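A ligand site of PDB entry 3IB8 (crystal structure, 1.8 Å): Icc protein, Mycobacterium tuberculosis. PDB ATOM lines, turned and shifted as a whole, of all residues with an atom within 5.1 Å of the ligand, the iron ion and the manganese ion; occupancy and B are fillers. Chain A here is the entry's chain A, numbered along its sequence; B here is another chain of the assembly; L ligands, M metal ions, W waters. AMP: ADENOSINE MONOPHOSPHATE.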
ATOM      1  N   ASP A  33      25.109 -29.992 -13.640  1.00  0.00           N
ATOM      2  CA  ASP A  33      24.715 -30.693 -12.421  1.00  0.00           C
ATOM      3  C   ASP A  33      25.304 -32.101 -12.355  1.00  0.00           C
ATOM      4  O   ASP A  33      24.586 -33.093 -12.232  1.00  0.00           O
ATOM      5  CB  ASP A  33      23.186 -30.697 -12.325  1.00  0.00           C
ATOM      6  CG  ASP A  33      22.632 -29.303 -12.032  1.00  0.00           C
ATOM      7  OD1 ASP A  33      22.553 -28.949 -10.850  1.00  0.00           O
ATOM      8  OD2 ASP A  33      22.306 -28.560 -12.974  1.00  0.00           O
ATOM      9  N   HIS A  35      27.472 -33.081  -9.926  1.00  0.00           N
ATOM     10  CA  HIS A  35      27.401 -33.455  -8.501  1.00  0.00           C
ATOM     11  C   HIS A  35      28.388 -34.556  -8.102  1.00  0.00           C
ATOM     12  O   HIS A  35      28.020 -35.490  -7.395  1.00  0.00           O
ATOM     13  CB  HIS A  35      25.960 -33.865  -8.135  1.00  0.00           C
ATOM     14  CG  HIS A  35      25.021 -32.708  -7.998  1.00  0.00           C
ATOM     15  ND1 HIS A  35      24.794 -32.077  -6.804  1.00  0.00           N
ATOM     16  CD2 HIS A  35      24.264 -32.059  -8.924  1.00  0.00           C
ATOM     17  CE1 HIS A  35      23.938 -31.087  -6.980  1.00  0.00           C
ATOM     18  NE2 HIS A  35      23.598 -31.056  -8.259  1.00  0.00           N
ATOM     19  N   TYR A  44      24.437 -39.463  -2.549  1.00  0.00           N
ATOM     20  CA  TYR A  44      23.304 -39.638  -1.633  1.00  0.00           C
ATOM     21  C   TYR A  44      23.008 -41.119  -1.344  1.00  0.00           C
ATOM     22  O   TYR A  44      21.869 -41.488  -1.045  1.00  0.00           O
ATOM     23  CB  TYR A  44      22.040 -38.885  -2.131  1.00  0.00           C
ATOM     24  CG  TYR A  44      22.269 -37.453  -2.587  1.00  0.00           C
ATOM     25  CD1 TYR A  44      23.368 -36.702  -2.164  1.00  0.00           C
ATOM     26  CD2 TYR A  44      21.353 -36.839  -3.448  1.00  0.00           C
ATOM     27  CE1 TYR A  44      23.562 -35.378  -2.596  1.00  0.00           C
ATOM     28  CE2 TYR A  44      21.527 -35.527  -3.886  1.00  0.00           C
ATOM     29  CZ  TYR A  44      22.633 -34.807  -3.448  1.00  0.00           C
ATOM     30  OH  TYR A  44      22.808 -33.513  -3.899  1.00  0.00           O
ATOM     31  N   ASP A  75      26.969 -26.723 -10.228  1.00  0.00           N
ATOM     32  CA  ASP A  75      26.827 -27.888  -9.334  1.00  0.00           C
ATOM     33  C   ASP A  75      27.749 -28.992  -9.832  1.00  0.00           C
ATOM     34  O   ASP A  75      27.328 -30.130 -10.082  1.00  0.00           O
ATOM     35  CB  ASP A  75      25.371 -28.380  -9.208  1.00  0.00           C
ATOM     36  CG  ASP A  75      24.526 -27.533  -8.261  1.00  0.00           C
ATOM     37  OD1 ASP A  75      25.055 -26.588  -7.627  1.00  0.00           O
ATOM     38  OD2 ASP A  75      23.317 -27.821  -8.139  1.00  0.00           O
ATOM     39  N   ASN A 109      25.191 -23.678  -6.762  1.00  0.00           N
ATOM     40  CA  ASN A 109      25.041 -23.515  -5.303  1.00  0.00           C
ATOM     41  C   ASN A 109      25.817 -24.549  -4.477  1.00  0.00           C
ATOM     42  O   ASN A 109      26.218 -24.256  -3.352  1.00  0.00           O
ATOM     43  CB  ASN A 109      23.565 -23.478  -4.866  1.00  0.00           C
ATOM     44  CG  ASN A 109      22.750 -24.634  -5.430  1.00  0.00           C
ATOM     45  OD1 ASN A 109      22.641 -24.790  -6.651  1.00  0.00           O
ATOM     46  ND2 ASN A 109      22.146 -25.432  -4.557  1.00  0.00           N
ATOM     47  N   HIS A 110      26.023 -25.747  -5.032  1.00  0.00           N
ATOM     48  CA  HIS A 110      26.759 -26.800  -4.331  1.00  0.00           C
ATOM     49  C   HIS A 110      28.288 -26.619  -4.379  1.00  0.00           C
ATOM     50  O   HIS A 110      29.021 -27.199  -3.586  1.00  0.00           O
ATOM     51  CB  HIS A 110      26.418 -28.164  -4.917  1.00  0.00           C
ATOM     52  CG  HIS A 110      25.076 -28.658  -4.496  1.00  0.00           C
ATOM     53  ND1 HIS A 110      24.911 -29.647  -3.552  1.00  0.00           N
ATOM     54  CD2 HIS A 110      23.826 -28.294  -4.882  1.00  0.00           C
ATOM     55  CE1 HIS A 110      23.626 -29.870  -3.360  1.00  0.00           C
ATOM     56  NE2 HIS A 110      22.941 -29.060  -4.148  1.00  0.00           N
ATOM     57  N   HIS A 181      23.932 -20.714 -13.390  1.00  0.00           N
ATOM     58  CA  HIS A 181      23.322 -21.887 -12.776  1.00  0.00           C
ATOM     59  C   HIS A 181      21.801 -21.757 -12.583  1.00  0.00           C
ATOM     60  O   HIS A 181      21.030 -22.540 -13.156  1.00  0.00           O
ATOM     61  CB  HIS A 181      23.992 -22.230 -11.440  1.00  0.00           C
ATOM     62  CG  HIS A 181      23.532 -23.519 -10.846  1.00  0.00           C
ATOM     63  ND1 HIS A 181      23.716 -24.741 -11.471  1.00  0.00           N
ATOM     64  CD2 HIS A 181      22.916 -23.789  -9.669  1.00  0.00           C
ATOM     65  CE1 HIS A 181      23.225 -25.699 -10.704  1.00  0.00           C
ATOM     66  NE2 HIS A 181      22.721 -25.143  -9.610  1.00  0.00           N
ATOM     67  N   LEU A 189       7.958 -27.344 -10.536  1.00  0.00           N
ATOM     68  CA  LEU A 189       8.071 -27.958  -9.210  1.00  0.00           C
ATOM     69  C   LEU A 189       8.030 -26.909  -8.100  1.00  0.00           C
ATOM     70  O   LEU A 189       8.856 -25.985  -8.066  1.00  0.00           O
ATOM     71  CB  LEU A 189       9.351 -28.793  -9.117  1.00  0.00           C
ATOM     72  CG  LEU A 189       9.508 -29.905 -10.156  1.00  0.00           C
ATOM     73  CD1 LEU A 189      10.869 -30.570  -9.995  1.00  0.00           C
ATOM     74  CD2 LEU A 189       8.385 -30.935 -10.042  1.00  0.00           C
ATOM     75  N   MET A 191       8.755 -26.889  -4.887  1.00  0.00           N
ATOM     76  CA  MET A 191       9.937 -26.791  -4.001  1.00  0.00           C
ATOM     77  C   MET A 191      11.043 -25.911  -4.583  1.00  0.00           C
ATOM     78  O   MET A 191      11.852 -25.349  -3.847  1.00  0.00           O
ATOM     79  CB  MET A 191      10.505 -28.177  -3.680  1.00  0.00           C
ATOM     80  CG  MET A 191       9.770 -28.929  -2.581  1.00  0.00           C
ATOM     81  SD  MET A 191       9.670 -28.037  -1.011  1.00  0.00           S
ATOM     82  CE  MET A 191      11.407 -27.749  -0.607  1.00  0.00           C
ATOM     83  N   ALA A 192      11.087 -25.809  -5.915  1.00  0.00           N
ATOM     84  CA  ALA A 192      12.100 -24.989  -6.567  1.00  0.00           C
ATOM     85  C   ALA A 192      12.079 -23.513  -6.119  1.00  0.00           C
ATOM     86  O   ALA A 192      13.136 -22.858  -6.124  1.00  0.00           O
ATOM     87  CB  ALA A 192      11.983 -25.100  -8.105  1.00  0.00           C
ATOM     88  N   THR A 194      11.946 -22.253  -3.237  1.00  0.00           N
ATOM     89  CA  THR A 194      12.753 -22.030  -2.020  1.00  0.00           C
ATOM     90  C   THR A 194      14.192 -21.673  -2.364  1.00  0.00           C
ATOM     91  O   THR A 194      14.885 -21.051  -1.558  1.00  0.00           O
ATOM     92  CB  THR A 194      12.785 -23.268  -1.064  1.00  0.00           C
ATOM     93  OG1 THR A 194      13.370 -24.386  -1.760  1.00  0.00           O
ATOM     94  CG2 THR A 194      11.386 -23.623  -0.578  1.00  0.00           C
ATOM     95  N   VAL A 195      14.647 -22.088  -3.540  1.00  0.00           N
ATOM     96  CA  VAL A 195      16.042 -21.922  -3.936  1.00  0.00           C
ATOM     97  C   VAL A 195      16.177 -21.338  -5.352  1.00  0.00           C
ATOM     98  O   VAL A 195      17.199 -21.514  -6.012  1.00  0.00           O
ATOM     99  CB  VAL A 195      16.858 -23.266  -3.811  1.00  0.00           C
ATOM    100  CG1 VAL A 195      17.052 -23.665  -2.346  1.00  0.00           C
ATOM    101  CG2 VAL A 195      16.178 -24.392  -4.595  1.00  0.00           C
ATOM    102  N   HIS A 219      20.440 -26.340 -12.544  1.00  0.00           N
ATOM    103  CA  HIS A 219      19.779 -26.207 -11.222  1.00  0.00           C
ATOM    104  C   HIS A 219      18.487 -27.020 -11.064  1.00  0.00           C
ATOM    105  O   HIS A 219      18.265 -27.602 -10.005  1.00  0.00           O
ATOM    106  CB  HIS A 219      19.581 -24.720 -10.847  1.00  0.00           C
ATOM    107  CG  HIS A 219      19.127 -24.479  -9.436  1.00  0.00           C
ATOM    108  ND1 HIS A 219      19.855 -24.879  -8.335  1.00  0.00           N
ATOM    109  CD2 HIS A 219      18.044 -23.823  -8.962  1.00  0.00           C
ATOM    110  CE1 HIS A 219      19.229 -24.489  -7.234  1.00  0.00           C
ATOM    111  NE2 HIS A 219      18.126 -23.846  -7.585  1.00  0.00           N
ATOM    112  N   LEU A 220      17.659 -27.093 -12.095  1.00  0.00           N
ATOM    113  CA  LEU A 220      16.342 -27.706 -11.955  1.00  0.00           C
ATOM    114  C   LEU A 220      16.353 -29.241 -12.027  1.00  0.00           C
ATOM    115  O   LEU A 220      15.431 -29.897 -11.530  1.00  0.00           O
ATOM    116  CB  LEU A 220      15.356 -27.110 -12.974  1.00  0.00           C
ATOM    117  CG  LEU A 220      15.033 -25.626 -12.734  1.00  0.00           C
ATOM    118  CD1 LEU A 220      14.089 -25.099 -13.801  1.00  0.00           C
ATOM    119  CD2 LEU A 220      14.404 -25.448 -11.349  1.00  0.00           C
ATOM    120  N   HIS A 221      17.398 -29.809 -12.640  1.00  0.00           N
ATOM    121  CA  HIS A 221      17.505 -31.270 -12.845  1.00  0.00           C
ATOM    122  C   HIS A 221      16.327 -31.850 -13.660  1.00  0.00           C
ATOM    123  O   HIS A 221      15.902 -32.989 -13.442  1.00  0.00           O
ATOM    124  CB  HIS A 221      17.627 -32.018 -11.502  1.00  0.00           C
ATOM    125  CG  HIS A 221      18.929 -31.792 -10.776  1.00  0.00           C
ATOM    126  ND1 HIS A 221      19.692 -32.830 -10.281  1.00  0.00           N
ATOM    127  CD2 HIS A 221      19.613 -30.653 -10.493  1.00  0.00           C
ATOM    128  CE1 HIS A 221      20.770 -32.344  -9.695  1.00  0.00           C
ATOM    129  NE2 HIS A 221      20.748 -31.028  -9.804  1.00  0.00           N
ATOM    130  N   TYR A 241      21.230 -37.404 -11.556  1.00  0.00           N
ATOM    131  CA  TYR A 241      19.867 -37.875 -11.274  1.00  0.00           C
ATOM    132  C   TYR A 241      18.934 -36.739 -11.676  1.00  0.00           C
ATOM    133  O   TYR A 241      19.354 -35.574 -11.732  1.00  0.00           O
ATOM    134  CB  TYR A 241      19.682 -38.234  -9.784  1.00  0.00           C
ATOM    135  CG  TYR A 241      19.539 -37.022  -8.886  1.00  0.00           C
ATOM    136  CD1 TYR A 241      18.261 -36.482  -8.627  1.00  0.00           C
ATOM    137  CD2 TYR A 241      20.656 -36.389  -8.343  1.00  0.00           C
ATOM    138  CE1 TYR A 241      18.123 -35.342  -7.823  1.00  0.00           C
ATOM    139  CE2 TYR A 241      20.521 -35.241  -7.536  1.00  0.00           C
ATOM    140  CZ  TYR A 241      19.242 -34.736  -7.272  1.00  0.00           C
ATOM    141  OH  TYR A 241      19.077 -33.608  -6.498  1.00  0.00           O
ATOM    142  N   GLN A 243      14.704 -34.958 -11.953  1.00  0.00           N
ATOM    143  CA  GLN A 243      13.381 -34.888 -11.339  1.00  0.00           C
ATOM    144  C   GLN A 243      12.361 -35.717 -12.126  1.00  0.00           C
ATOM    145  O   GLN A 243      12.337 -35.703 -13.353  1.00  0.00           O
ATOM    146  CB  GLN A 243      12.935 -33.432 -11.225  1.00  0.00           C
ATOM    147  CG  GLN A 243      13.771 -32.636 -10.212  1.00  0.00           C
ATOM    148  CD  GLN A 243      13.560 -33.131  -8.793  1.00  0.00           C
ATOM    149  OE1 GLN A 243      12.519 -33.692  -8.455  1.00  0.00           O
ATOM    150  NE2 GLN A 243      14.561 -32.921  -7.940  1.00  0.00           N
ATOM    151  N   THR A 252       7.944 -33.482  -5.041  1.00  0.00           N
ATOM    152  CA  THR A 252       9.197 -33.604  -5.779  1.00  0.00           C
ATOM    153  C   THR A 252       9.864 -34.965  -5.485  1.00  0.00           C
ATOM    154  O   THR A 252       9.864 -35.441  -4.350  1.00  0.00           O
ATOM    155  CB  THR A 252      10.175 -32.421  -5.528  1.00  0.00           C
ATOM    156  OG1 THR A 252      11.427 -32.657  -6.200  1.00  0.00           O
ATOM    157  CG2 THR A 252      10.461 -32.254  -4.064  1.00  0.00           C
ATOM    158  N   THR B 286      15.846 -37.076  -1.110  1.00  0.00           N
ATOM    159  CA  THR B 286      14.631 -37.207  -0.315  1.00  0.00           C
ATOM    160  C   THR B 286      13.376 -36.961  -1.143  1.00  0.00           C
ATOM    161  O   THR B 286      13.296 -35.973  -1.878  1.00  0.00           O
ATOM    162  CB  THR B 286      14.672 -36.239   0.892  1.00  0.00           C
ATOM    163  OG1 THR B 286      15.776 -36.594   1.729  1.00  0.00           O
ATOM    164  CG2 THR B 286      13.392 -36.303   1.708  1.00  0.00           C
ATOM    165  N   VAL B 288       9.827 -35.567  -1.447  1.00  0.00           N
ATOM    166  CA  VAL B 288       8.998 -34.576  -0.739  1.00  0.00           C
ATOM    167  C   VAL B 288       7.549 -34.681  -1.206  1.00  0.00           C
ATOM    168  O   VAL B 288       7.237 -34.436  -2.378  1.00  0.00           O
ATOM    169  CB  VAL B 288       9.518 -33.123  -0.959  1.00  0.00           C
ATOM    170  CG1 VAL B 288       8.723 -32.142  -0.100  1.00  0.00           C
ATOM    171  CG2 VAL B 288      11.010 -33.030  -0.644  1.00  0.00           C
ATOM    172  N   LYS B 296       7.317 -26.843   3.886  1.00  0.00           N
ATOM    173  CA  LYS B 296       8.701 -26.384   3.679  1.00  0.00           C
ATOM    174  C   LYS B 296       8.778 -25.004   3.033  1.00  0.00           C
ATOM    175  O   LYS B 296       9.592 -24.160   3.445  1.00  0.00           O
ATOM    176  CB  LYS B 296       9.505 -27.397   2.835  1.00  0.00           C
ATOM    177  CG  LYS B 296       9.997 -28.619   3.604  1.00  0.00           C
ATOM    178  CD  LYS B 296      10.562 -29.675   2.653  1.00  0.00           C
ATOM    179  CE  LYS B 296      10.921 -30.958   3.366  1.00  0.00           C
ATOM    180  NZ  LYS B 296      12.185 -30.829   4.156  1.00  0.00           N
HETATM  181  P   AMP L   1      20.462 -28.731  -6.132  1.00  0.00           P
HETATM  182  O1P AMP L   1      20.838 -27.277  -6.273  1.00  0.00           O
HETATM  183  O2P AMP L   1      20.364 -29.104  -4.645  1.00  0.00           O
HETATM  184  O3P AMP L   1      21.271 -29.752  -6.859  1.00  0.00           O
HETATM  185  O5' AMP L   1      18.970 -28.889  -6.688  1.00  0.00           O
HETATM  186  C5' AMP L   1      18.008 -27.851  -6.542  1.00  0.00           C
HETATM  187  C4' AMP L   1      16.703 -28.341  -7.132  1.00  0.00           C
HETATM  188  O4' AMP L   1      16.316 -29.525  -6.437  1.00  0.00           O
HETATM  189  C3' AMP L   1      15.615 -27.313  -6.901  1.00  0.00           C
HETATM  190  O3' AMP L   1      15.483 -26.478  -8.051  1.00  0.00           O
HETATM  191  C2' AMP L   1      14.383 -28.148  -6.590  1.00  0.00           C
HETATM  192  O2' AMP L   1      13.572 -28.270  -7.764  1.00  0.00           O
HETATM  193  C1' AMP L   1      14.908 -29.517  -6.197  1.00  0.00           C
HETATM  194  N9  AMP L   1      14.675 -29.888  -4.778  1.00  0.00           N
HETATM  195  C8  AMP L   1      14.295 -31.126  -4.364  1.00  0.00           C
HETATM  196  N7  AMP L   1      14.159 -31.185  -3.006  1.00  0.00           N
HETATM  197  C5  AMP L   1      14.466 -29.963  -2.531  1.00  0.00           C
HETATM  198  C6  AMP L   1      14.529 -29.324  -1.194  1.00  0.00           C
HETATM  199  N6  AMP L   1      14.228 -30.002  -0.056  1.00  0.00           N
HETATM  200  N1  AMP L   1      14.899 -28.014  -1.145  1.00  0.00           N
HETATM  201  C2  AMP L   1      15.194 -27.311  -2.247  1.00  0.00           C
HETATM  202  N3  AMP L   1      15.156 -27.827  -3.479  1.00  0.00           N
HETATM  203  C4  AMP L   1      14.804 -29.119  -3.699  1.00  0.00           C
HETATM  204 FE    FE M   1      22.101 -29.548  -8.900  1.00  0.00          FE
HETATM  205 MN    MN M   2      21.703 -26.247  -7.973  1.00  0.00          MN
HETATM  206  O   HOH W   1      14.184 -29.250   2.831  1.00  0.00           O
HETATM  207  O   HOH W   2      18.294 -30.662  -3.944  1.00  0.00           O
HETATM  208  O   HOH W   3      15.048 -25.904   0.391  1.00  0.00           O
HETATM  209  O   HOH W   4      15.144 -33.946  -5.161  1.00  0.00           O
HETATM  210  O   HOH W   5      21.287 -32.427  -5.959  1.00  0.00           O
HETATM  211  O   HOH W   6      17.997 -26.434  -0.488  1.00  0.00           O
HETATM  212  O   HOH W   7      14.548 -33.213  -1.471  1.00  0.00           O
HETATM  213  O   HOH W   8      20.701 -28.088  -8.897  1.00  0.00           O
HETATM  214  O   HOH W   9      17.429 -31.642  -7.807  1.00  0.00           O
HETATM  215  O   HOH W  10      15.063 -23.510  -7.880  1.00  0.00           O
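NE2 of His 110 sits at hydrogen-bond distance from O2P of the ligand (2.6 Å).
The backbone carbonyl oxygen of Tyr 241 sits at hydrogen-bond distance from a ring nitrogen (ND1) of His 221, 3.1 Å away. NE2 of His 219 lies within hydrogen-bond range of O of Val 195 (3.0 Å). The backbone carbonyl oxygen (O) of His 221 sits at hydrogen-bond distance from the backbone NH (N) of Gln 243 (2.7 Å). The side-chain carboxylate (OD2) of Asp 33 sits at hydrogen-bond distance from the backbone NH (N) of His 219. The backbone NH of His 110 is in hydrogen-bond range of the side-chain carboxylate of Asp 75 (2.9 Å). The side-chain hydroxyl (OG1) of Thr 194 is in hydrogen-bond range of the backbone carbonyl oxygen (O) of Met 191, 2.8 Å away. OE1 of Gln 243 lies within hydrogen-bond range of OG1 of Thr 252 (2.7 Å). O of Thr 252 sits at hydrogen-bond distance from N of Val 288 of chain B (2.9 Å).
Merely in contact with the ligand: Thr 194 (3.5 Å), Met 191 (3.5 Å), Ala 192 (3.6 Å), Leu 220 (3.6 Å), Thr 252 (3.7 Å), Val 195 (3.8 Å) and Gln 243 (3.8 Å). The nearest printed residue that does not touch the ligand is Leu 189 (4.2 Å).
Four residues have an atom within 4 Å of the manganese ion: Asp 75, Asn 109, His 181 and His 219.
Water W8 binds the iron ion, at 2.0 Å. OD1 of Asp 33 binds the iron ion (2.1 Å). A ring nitrogen (NE2) of His 221 is bound to the iron ion, 2.2 Å away. O3P of the ligand is bound to the iron ion, 2.2 Å away. NE2 of His 35 binds the iron ion, at 2.2 Å. OD2 of Asp 75 is bound to the iron ion (2.2 Å). The iron ion has six donor atoms within binding distance.
The manganese ion is bound by O1P of the ligand, OD1 of Asn 109, NE2 of His 181, OD2 of Asp 75, water W8 and ND1 of His 219. The manganese ion has six donor atoms within binding distance.
Water W8 lies within hydrogen-bond range of O of His 219 (2.7 Å) and O5' of the ligand (2.9 Å). Water W3 bridges a nitrogen (N1) of the ligand and the side-chain hydroxyl of Thr 194. Water W9 lies within hydrogen-bond range of an oxygen (O4') of the ligand (2.8 Å), the side-chain hydroxyl (OH) of Tyr 241 (2.9 Å) and the side-chain amide nitrogen (NE2) of Gln 243 (3.1 Å). Water W5 lies within hydrogen-bond range of OH of Tyr 241 (2.6 Å) and OH of Tyr 44 (2.8 Å). Water W1 bridges NZ of Lys 296 of chain B (2.9 Å) and N6 of the ligand (3.0 Å). Water W10 lies within hydrogen-bond range of O of Ala 192 (2.7 Å), O3' of the ligand (3.0 Å), NE2 of His 219 (3.1 Å) and O of Val 195 (3.5 Å).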
